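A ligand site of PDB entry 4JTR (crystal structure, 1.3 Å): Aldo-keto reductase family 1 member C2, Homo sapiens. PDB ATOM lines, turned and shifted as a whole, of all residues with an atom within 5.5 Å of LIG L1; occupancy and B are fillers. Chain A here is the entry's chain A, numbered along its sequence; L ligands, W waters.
Water W1 lies within hydrogen-bond range of O1 of LIG L1 (2.5 Å) and NE2 of His 222 (2.8 Å).
Water W2 bridges O1 of LIG L1 (2.5 Å) and OH of Tyr 55 (3.5 Å).
OH of Tyr 55 is in hydrogen-bond range of NZ of Lys 84, at 3.1 Å.
The backbone carbonyl oxygen of Val 128 is in hydrogen-bond range of the indole nitrogen of Trp 86 (2.8 Å).
The side-chain carboxylate of Glu 224 is in hydrogen-bond range of the side-chain hydroxyl of Tyr 24.
The side-chain hydroxyl (OH) of Tyr 55 lies within hydrogen-bond range of an oxygen (O2) of LIG L1.
A ring nitrogen (NE2) of His 117 sits at hydrogen-bond distance from an oxygen (O2) of LIG L1.
The backbone NH (N) of Tyr 24 sits at hydrogen-bond distance from an oxygen (O12) of LG2 L2 (3.1 Å).
O8 of LG2 L2 is in hydrogen-bond range of N of His 222 (3.2 Å).
Tyr 24 touches LIG L1 (OH to C5, 3.7 Å).
Val 54 touches LIG L1.
Trp 86 touches LIG L1 (CH2 to C9, 3.6 Å).
CZ2 of Trp 227 touches C5 of LIG L1 (3.5 Å).
Leu 308 touches LIG L1.
Of the 15 residues printed, 7 come within 4 Å of LIG L1.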
ATOM      1  N   TYR A  24       8.016   2.059   3.910  1.00  0.00           N
ATOM      2  CA  TYR A  24       7.723   0.762   4.547  1.00  0.00           C
ATOM      3  C   TYR A  24       7.184   1.011   5.967  1.00  0.00           C
ATOM      4  O   TYR A  24       7.710   1.885   6.716  1.00  0.00           O
ATOM      5  CB  TYR A  24       8.983  -0.036   4.717  1.00  0.00           C
ATOM      6  CG  TYR A  24       8.670  -1.391   5.411  1.00  0.00           C
ATOM      7  CD1 TYR A  24       7.965  -2.381   4.750  1.00  0.00           C
ATOM      8  CD2 TYR A  24       8.904  -1.561   6.755  1.00  0.00           C
ATOM      9  CE1 TYR A  24       7.647  -3.570   5.383  1.00  0.00           C
ATOM     10  CE2 TYR A  24       8.581  -2.748   7.404  1.00  0.00           C
ATOM     11  CZ  TYR A  24       7.988  -3.763   6.697  1.00  0.00           C
ATOM     12  OH  TYR A  24       7.614  -4.896   7.414  1.00  0.00           O
ATOM     13  N   VAL A  54       7.477  -5.585  -2.386  1.00  0.00           N
ATOM     14  CA  VAL A  54       7.288  -6.405  -1.155  1.00  0.00           C
ATOM     15  C   VAL A  54       6.699  -5.610  -0.012  1.00  0.00           C
ATOM     16  O   VAL A  54       6.323  -6.174   1.013  1.00  0.00           O
ATOM     17  CB  VAL A  54       8.630  -7.148  -0.814  1.00  0.00           C
ATOM     18  CG1 VAL A  54       9.639  -6.182  -0.201  1.00  0.00           C
ATOM     19  CG2 VAL A  54       8.481  -8.448  -0.082  1.00  0.00           C
ATOM     20  N   TYR A  55       6.681  -4.292  -0.091  1.00  0.00           N
ATOM     21  CA  TYR A  55       6.097  -3.430   0.958  1.00  0.00           C
ATOM     22  C   TYR A  55       4.562  -3.500   0.997  1.00  0.00           C
ATOM     23  O   TYR A  55       3.964  -3.025   1.895  1.00  0.00           O
ATOM     24  CB  TYR A  55       6.547  -1.944   0.850  1.00  0.00           C
ATOM     25  CG  TYR A  55       8.050  -1.709   0.966  1.00  0.00           C
ATOM     26  CD1 TYR A  55       8.897  -2.723   1.330  1.00  0.00           C
ATOM     27  CD2 TYR A  55       8.606  -0.472   0.701  1.00  0.00           C
ATOM     28  CE1 TYR A  55      10.264  -2.549   1.424  1.00  0.00           C
ATOM     29  CE2 TYR A  55       9.964  -0.283   0.778  1.00  0.00           C
ATOM     30  CZ  TYR A  55      10.797  -1.309   1.127  1.00  0.00           C
ATOM     31  OH  TYR A  55      12.142  -1.146   1.197  1.00  0.00           O
ATOM     32  N   LYS A  84      11.269  -1.669  -6.408  1.00  0.00           N
ATOM     33  CA  LYS A  84      12.286  -2.729  -6.308  1.00  0.00           C
ATOM     34  C   LYS A  84      11.662  -4.083  -6.702  1.00  0.00           C
ATOM     35  O   LYS A  84      10.501  -4.335  -6.359  1.00  0.00           O
ATOM     36  CB  LYS A  84      12.819  -2.811  -4.870  1.00  0.00           C
ATOM     37  CG  LYS A  84      13.188  -1.487  -4.259  1.00  0.00           C
ATOM     38  CD  LYS A  84      13.928  -1.615  -2.914  1.00  0.00           C
ATOM     39  CE  LYS A  84      14.136  -0.293  -2.189  1.00  0.00           C
ATOM     40  NZ  LYS A  84      12.877   0.175  -1.498  1.00  0.00           N
ATOM     41  N   TRP A  86      11.405  -7.789  -6.373  1.00  0.00           N
ATOM     42  CA  TRP A  86      11.504  -8.754  -5.306  1.00  0.00           C
ATOM     43  C   TRP A  86      12.121 -10.078  -5.856  1.00  0.00           C
ATOM     44  O   TRP A  86      12.100 -10.355  -7.014  1.00  0.00           O
ATOM     45  CB  TRP A  86      10.143  -8.966  -4.555  1.00  0.00           C
ATOM     46  CG  TRP A  86      10.318  -9.808  -3.316  1.00  0.00           C
ATOM     47  CD1 TRP A  86       9.813 -11.052  -3.065  1.00  0.00           C
ATOM     48  CD2 TRP A  86      11.272  -9.565  -2.287  1.00  0.00           C
ATOM     49  NE1 TRP A  86      10.380 -11.580  -1.943  1.00  0.00           N
ATOM     50  CE2 TRP A  86      11.266 -10.690  -1.413  1.00  0.00           C
ATOM     51  CE3 TRP A  86      12.140  -8.485  -1.967  1.00  0.00           C
ATOM     52  CZ2 TRP A  86      12.108 -10.762  -0.281  1.00  0.00           C
ATOM     53  CZ3 TRP A  86      12.953  -8.551  -0.851  1.00  0.00           C
ATOM     54  CH2 TRP A  86      12.914  -9.712  -0.007  1.00  0.00           C
ATOM     55  N   HIS A 117      16.172  -5.792  -5.292  1.00  0.00           N
ATOM     56  CA  HIS A 117      15.990  -5.548  -3.881  1.00  0.00           C
ATOM     57  C   HIS A 117      17.001  -6.264  -2.965  1.00  0.00           C
ATOM     58  O   HIS A 117      17.479  -5.672  -1.995  1.00  0.00           O
ATOM     59  CB  HIS A 117      14.541  -5.876  -3.490  1.00  0.00           C
ATOM     60  CG  HIS A 117      14.015  -5.254  -2.267  1.00  0.00           C
ATOM     61  ND1 HIS A 117      12.693  -5.001  -2.029  1.00  0.00           N
ATOM     62  CD2 HIS A 117      14.652  -4.791  -1.167  1.00  0.00           C
ATOM     63  CE1 HIS A 117      12.525  -4.469  -0.863  1.00  0.00           C
ATOM     64  NE2 HIS A 117      13.703  -4.306  -0.314  1.00  0.00           N
ATOM     65  N   VAL A 128       5.763 -13.977  -1.588  1.00  0.00           N
ATOM     66  CA  VAL A 128       7.023 -13.302  -1.538  1.00  0.00           C
ATOM     67  C   VAL A 128       8.089 -14.028  -0.676  1.00  0.00           C
ATOM     68  O   VAL A 128       9.249 -13.898  -0.983  1.00  0.00           O
ATOM     69  CB  VAL A 128       6.848 -11.883  -1.009  1.00  0.00           C
ATOM     70  CG1 VAL A 128       6.081 -10.961  -2.048  1.00  0.00           C
ATOM     71  CG2 VAL A 128       6.325 -11.733   0.412  1.00  0.00           C
ATOM     72  N   ILE A 129       7.658 -14.869   0.255  1.00  0.00           N
ATOM     73  CA  ILE A 129       8.626 -15.694   1.002  1.00  0.00           C
ATOM     74  C   ILE A 129       8.085 -17.149   0.870  1.00  0.00           C
ATOM     75  O   ILE A 129       7.417 -17.664   1.790  1.00  0.00           O
ATOM     76  CB  ILE A 129       8.730 -15.343   2.531  1.00  0.00           C
ATOM     77  CG1 ILE A 129       9.021 -13.867   2.771  1.00  0.00           C
ATOM     78  CG2 ILE A 129       9.762 -16.190   3.179  1.00  0.00           C
ATOM     79  CD1 ILE A 129      10.299 -13.387   2.213  1.00  0.00           C
ATOM     80  N   TYR A 216      19.550   3.504   3.843  1.00  0.00           N
ATOM     81  CA  TYR A 216      18.338   3.178   4.571  1.00  0.00           C
ATOM     82  C   TYR A 216      18.656   2.868   6.023  1.00  0.00           C
ATOM     83  O   TYR A 216      19.814   2.712   6.422  1.00  0.00           O
ATOM     84  CB  TYR A 216      17.598   2.008   3.912  1.00  0.00           C
ATOM     85  CG  TYR A 216      18.147   0.596   4.031  1.00  0.00           C
ATOM     86  CD1 TYR A 216      18.187  -0.078   5.289  1.00  0.00           C
ATOM     87  CD2 TYR A 216      18.577  -0.079   2.968  1.00  0.00           C
ATOM     88  CE1 TYR A 216      18.591  -1.398   5.325  1.00  0.00           C
ATOM     89  CE2 TYR A 216      18.920  -1.451   2.980  1.00  0.00           C
ATOM     90  CZ  TYR A 216      19.001  -2.057   4.205  1.00  0.00           C
ATOM     91  OH  TYR A 216      19.250  -3.406   4.287  1.00  0.00           O
ATOM     92  N   HIS A 222      13.187   0.880  11.494  1.00  0.00           N
ATOM     93  CA  HIS A 222      11.886   0.612  12.058  1.00  0.00           C
ATOM     94  C   HIS A 222      11.899  -0.215  13.341  1.00  0.00           C
ATOM     95  O   HIS A 222      10.902  -0.179  14.073  1.00  0.00           O
ATOM     96  CB  HIS A 222      10.933  -0.080  11.007  1.00  0.00           C
ATOM     97  CG  HIS A 222      11.541  -1.230  10.264  1.00  0.00           C
ATOM     98  ND1 HIS A 222      11.861  -2.442  10.856  1.00  0.00           N
ATOM     99  CD2 HIS A 222      11.854  -1.385   8.943  1.00  0.00           C
ATOM    100  CE1 HIS A 222      12.352  -3.278   9.952  1.00  0.00           C
ATOM    101  NE2 HIS A 222      12.385  -2.647   8.784  1.00  0.00           N
ATOM    102  N   GLU A 224      11.448  -3.321  13.663  1.00  0.00           N
ATOM    103  CA  GLU A 224      10.329  -4.279  13.674  1.00  0.00           C
ATOM    104  C   GLU A 224      10.860  -5.701  14.014  1.00  0.00           C
ATOM    105  O   GLU A 224      11.843  -6.179  13.421  1.00  0.00           O
ATOM    106  CB  GLU A 224       9.611  -4.313  12.291  1.00  0.00           C
ATOM    107  CG  GLU A 224       8.322  -5.103  12.261  1.00  0.00           C
ATOM    108  CD  GLU A 224       7.817  -5.392  10.866  1.00  0.00           C
ATOM    109  OE1 GLU A 224       8.461  -5.009   9.823  1.00  0.00           O
ATOM    110  OE2 GLU A 224       6.761  -6.067  10.857  1.00  0.00           O
ATOM    111  N   TRP A 227      12.654  -8.906  12.541  1.00  0.00           N
ATOM    112  CA  TRP A 227      13.684  -8.490  11.559  1.00  0.00           C
ATOM    113  C   TRP A 227      14.923  -7.826  12.178  1.00  0.00           C
ATOM    114  O   TRP A 227      16.051  -7.990  11.708  1.00  0.00           O
ATOM    115  CB  TRP A 227      13.052  -7.576  10.484  1.00  0.00           C
ATOM    116  CG  TRP A 227      11.846  -8.186   9.910  1.00  0.00           C
ATOM    117  CD1 TRP A 227      10.563  -7.828  10.132  1.00  0.00           C
ATOM    118  CD2 TRP A 227      11.816  -9.302   9.022  1.00  0.00           C
ATOM    119  NE1 TRP A 227       9.698  -8.677   9.419  1.00  0.00           N
ATOM    120  CE2 TRP A 227      10.444  -9.574   8.720  1.00  0.00           C
ATOM    121  CE3 TRP A 227      12.800 -10.093   8.450  1.00  0.00           C
ATOM    122  CZ2 TRP A 227      10.058 -10.617   7.850  1.00  0.00           C
ATOM    123  CZ3 TRP A 227      12.426 -11.114   7.623  1.00  0.00           C
ATOM    124  CH2 TRP A 227      11.063 -11.376   7.304  1.00  0.00           C
ATOM    125  N   LEU A 306      19.708  -4.670  10.093  1.00  0.00           N
ATOM    126  CA  LEU A 306      18.934  -5.432   9.140  1.00  0.00           C
ATOM    127  C   LEU A 306      19.774  -6.546   8.544  1.00  0.00           C
ATOM    128  O   LEU A 306      20.513  -6.327   7.621  1.00  0.00           O
ATOM    129  CB  LEU A 306      18.391  -4.520   8.050  1.00  0.00           C
ATOM    130  CG  LEU A 306      17.448  -5.246   7.087  1.00  0.00           C
ATOM    131  CD1 LEU A 306      18.292  -6.102   6.174  1.00  0.00           C
ATOM    132  CD2 LEU A 306      16.348  -6.055   7.821  1.00  0.00           C
ATOM    133  N   LEU A 308      18.304  -9.743   7.531  1.00  0.00           N
ATOM    134  CA  LEU A 308      17.495 -10.551   6.647  1.00  0.00           C
ATOM    135  C   LEU A 308      18.029 -11.991   6.710  1.00  0.00           C
ATOM    136  O   LEU A 308      18.160 -12.673   5.688  1.00  0.00           O
ATOM    137  CB  LEU A 308      17.547  -9.971   5.211  1.00  0.00           C
ATOM    138  CG  LEU A 308      16.970  -8.541   5.264  1.00  0.00           C
ATOM    139  CD1 LEU A 308      17.301  -7.706   4.033  1.00  0.00           C
ATOM    140  CD2 LEU A 308      15.507  -8.734   5.521  1.00  0.00           C
ATOM    141  N   PHE A 311      17.345 -15.340   4.805  1.00  0.00           N
ATOM    142  CA  PHE A 311      17.941 -15.647   3.522  1.00  0.00           C
ATOM    143  C   PHE A 311      19.420 -15.998   3.556  1.00  0.00           C
ATOM    144  O   PHE A 311      20.070 -16.113   2.531  1.00  0.00           O
ATOM    145  CB  PHE A 311      17.737 -14.519   2.514  1.00  0.00           C
ATOM    146  CG  PHE A 311      16.329 -14.037   2.435  1.00  0.00           C
ATOM    147  CD1 PHE A 311      15.325 -14.853   1.887  1.00  0.00           C
ATOM    148  CD2 PHE A 311      15.997 -12.776   2.822  1.00  0.00           C
ATOM    149  CE1 PHE A 311      14.019 -14.434   1.813  1.00  0.00           C
ATOM    150  CE2 PHE A 311      14.675 -12.352   2.747  1.00  0.00           C
ATOM    151  CZ  PHE A 311      13.716 -13.157   2.218  1.00  0.00           C
HETATM  152  C1  LIG L   1      13.252  -4.046   3.234  1.00  0.00           C
HETATM  153  C2  LIG L   1       8.719  -8.428   3.350  1.00  0.00           C
HETATM  154  C3  LIG L   1       8.613  -9.206   4.675  1.00  0.00           C
HETATM  155  C4  LIG L   1       7.377 -10.105   4.542  1.00  0.00           C
HETATM  156  C5  LIG L   1       8.381  -8.215   5.883  1.00  0.00           C
HETATM  157  C6  LIG L   1      13.537  -5.524   3.163  1.00  0.00           C
HETATM  158  C7  LIG L   1      14.413  -5.898   4.293  1.00  0.00           C
HETATM  159  C8  LIG L   1      12.277  -6.251   3.231  1.00  0.00           C
HETATM  160  C9  LIG L   1      12.217  -7.521   2.801  1.00  0.00           C
HETATM  161  C10 LIG L   1      11.032  -8.216   2.869  1.00  0.00           C
HETATM  162  C11 LIG L   1       9.905  -7.664   3.339  1.00  0.00           C
HETATM  163  C12 LIG L   1       9.892  -6.331   3.767  1.00  0.00           C
HETATM  164  C13 LIG L   1      11.078  -5.590   3.729  1.00  0.00           C
HETATM  165  O1  LIG L   1      12.915  -3.564   4.293  1.00  0.00           O
HETATM  166  O2  LIG L   1      13.189  -3.266   2.167  1.00  0.00           O
HETATM  167  P1  LG2 L   2      14.304   4.967   9.324  1.00  0.00           P
HETATM  168  O1  LG2 L   2      15.595   4.607   9.837  1.00  0.00           O
HETATM  169  O2  LG2 L   2      14.130   5.982   8.280  1.00  0.00           O
HETATM  170  O3  LG2 L   2      13.463   5.319  10.639  1.00  0.00           O
HETATM  171  C1  LG2 L   2      12.103   5.250  10.740  1.00  0.00           C
HETATM  172  C2  LG2 L   2      11.880   5.379  12.264  1.00  0.00           C
HETATM  173  O4  LG2 L   2      12.379   6.706  12.757  1.00  0.00           O
HETATM  174  C3  LG2 L   2      10.371   5.296  12.197  1.00  0.00           C
HETATM  175  O5  LG2 L   2       9.945   4.561  13.324  1.00  0.00           O
HETATM  176  C4  LG2 L   2       9.989   6.804  12.454  1.00  0.00           C
HETATM  177  O6  LG2 L   2       8.861   6.837  13.303  1.00  0.00           O
HETATM  178  C5  LG2 L   2      11.196   7.385  13.148  1.00  0.00           C
HETATM  179  N1  LG2 L   2      11.469   8.846  12.817  1.00  0.00           N
HETATM  180  C6  LG2 L   2      11.368   9.400  11.612  1.00  0.00           C
HETATM  181  N2  LG2 L   2      11.750  10.686  11.651  1.00  0.00           N
HETATM  182  C7  LG2 L   2      12.067  10.968  12.957  1.00  0.00           C
HETATM  183  C8  LG2 L   2      12.511  12.127  13.591  1.00  0.00           C
HETATM  184  N3  LG2 L   2      12.613  13.310  13.001  1.00  0.00           N
HETATM  185  N4  LG2 L   2      12.688  12.082  14.942  1.00  0.00           N
HETATM  186  C9  LG2 L   2      12.569  10.831  15.536  1.00  0.00           C
HETATM  187  N5  LG2 L   2      12.106   9.690  15.004  1.00  0.00           N
HETATM  188  C10 LG2 L   2      11.927   9.772  13.647  1.00  0.00           C
HETATM  189  O7  LG2 L   2      13.388   3.661   8.935  1.00  0.00           O
HETATM  190  P2  LG2 L   2      13.493   2.452   7.938  1.00  0.00           P
HETATM  191  O8  LG2 L   2      14.159   1.284   8.474  1.00  0.00           O
HETATM  192  O9  LG2 L   2      12.009   2.321   7.550  1.00  0.00           O
HETATM  193  O10 LG2 L   2      14.262   2.956   6.660  1.00  0.00           O
HETATM  194  C11 LG2 L   2      13.696   3.993   5.850  1.00  0.00           C
HETATM  195  C12 LG2 L   2      13.270   3.504   4.509  1.00  0.00           C
HETATM  196  O11 LG2 L   2      14.328   2.860   3.780  1.00  0.00           O
HETATM  197  C13 LG2 L   2      12.123   2.373   4.432  1.00  0.00           C
HETATM  198  O12 LG2 L   2      10.865   2.930   4.786  1.00  0.00           O
HETATM  199  C14 LG2 L   2      12.264   1.839   3.001  1.00  0.00           C
HETATM  200  O13 LG2 L   2      11.735   2.814   2.157  1.00  0.00           O
HETATM  201  C15 LG2 L   2      13.852   1.818   2.899  1.00  0.00           C
HETATM  202  N6  LG2 L   2      14.464   0.568   3.302  1.00  0.00           N
HETATM  203  C16 LG2 L   2      14.957  -0.258   2.324  1.00  0.00           C
HETATM  204  C17 LG2 L   2      15.522  -1.458   2.619  1.00  0.00           C
HETATM  205  C18 LG2 L   2      16.100  -2.300   1.627  1.00  0.00           C
HETATM  206  O14 LG2 L   2      16.407  -3.520   1.795  1.00  0.00           O
HETATM  207  N7  LG2 L   2      16.421  -1.754   0.427  1.00  0.00           N
HETATM  208  C19 LG2 L   2      15.611  -1.860   3.975  1.00  0.00           C
HETATM  209  C20 LG2 L   2      15.175  -1.025   4.989  1.00  0.00           C
HETATM  210  C21 LG2 L   2      14.600   0.229   4.695  1.00  0.00           C
HETATM  211  P3  LG2 L   2       7.570   7.668  12.838  1.00  0.00           P
HETATM  212  O15 LG2 L   2       7.076   7.008  11.525  1.00  0.00           O
HETATM  213  O16 LG2 L   2       6.620   7.409  13.993  1.00  0.00           O
HETATM  214  O17 LG2 L   2       7.999   9.119  12.655  1.00  0.00           O
HETATM  215  O   HOH W   1      12.803  -4.316   6.626  1.00  0.00           O
HETATM  216  O   HOH W   2      11.968  -1.328   4.688  1.00  0.00           O
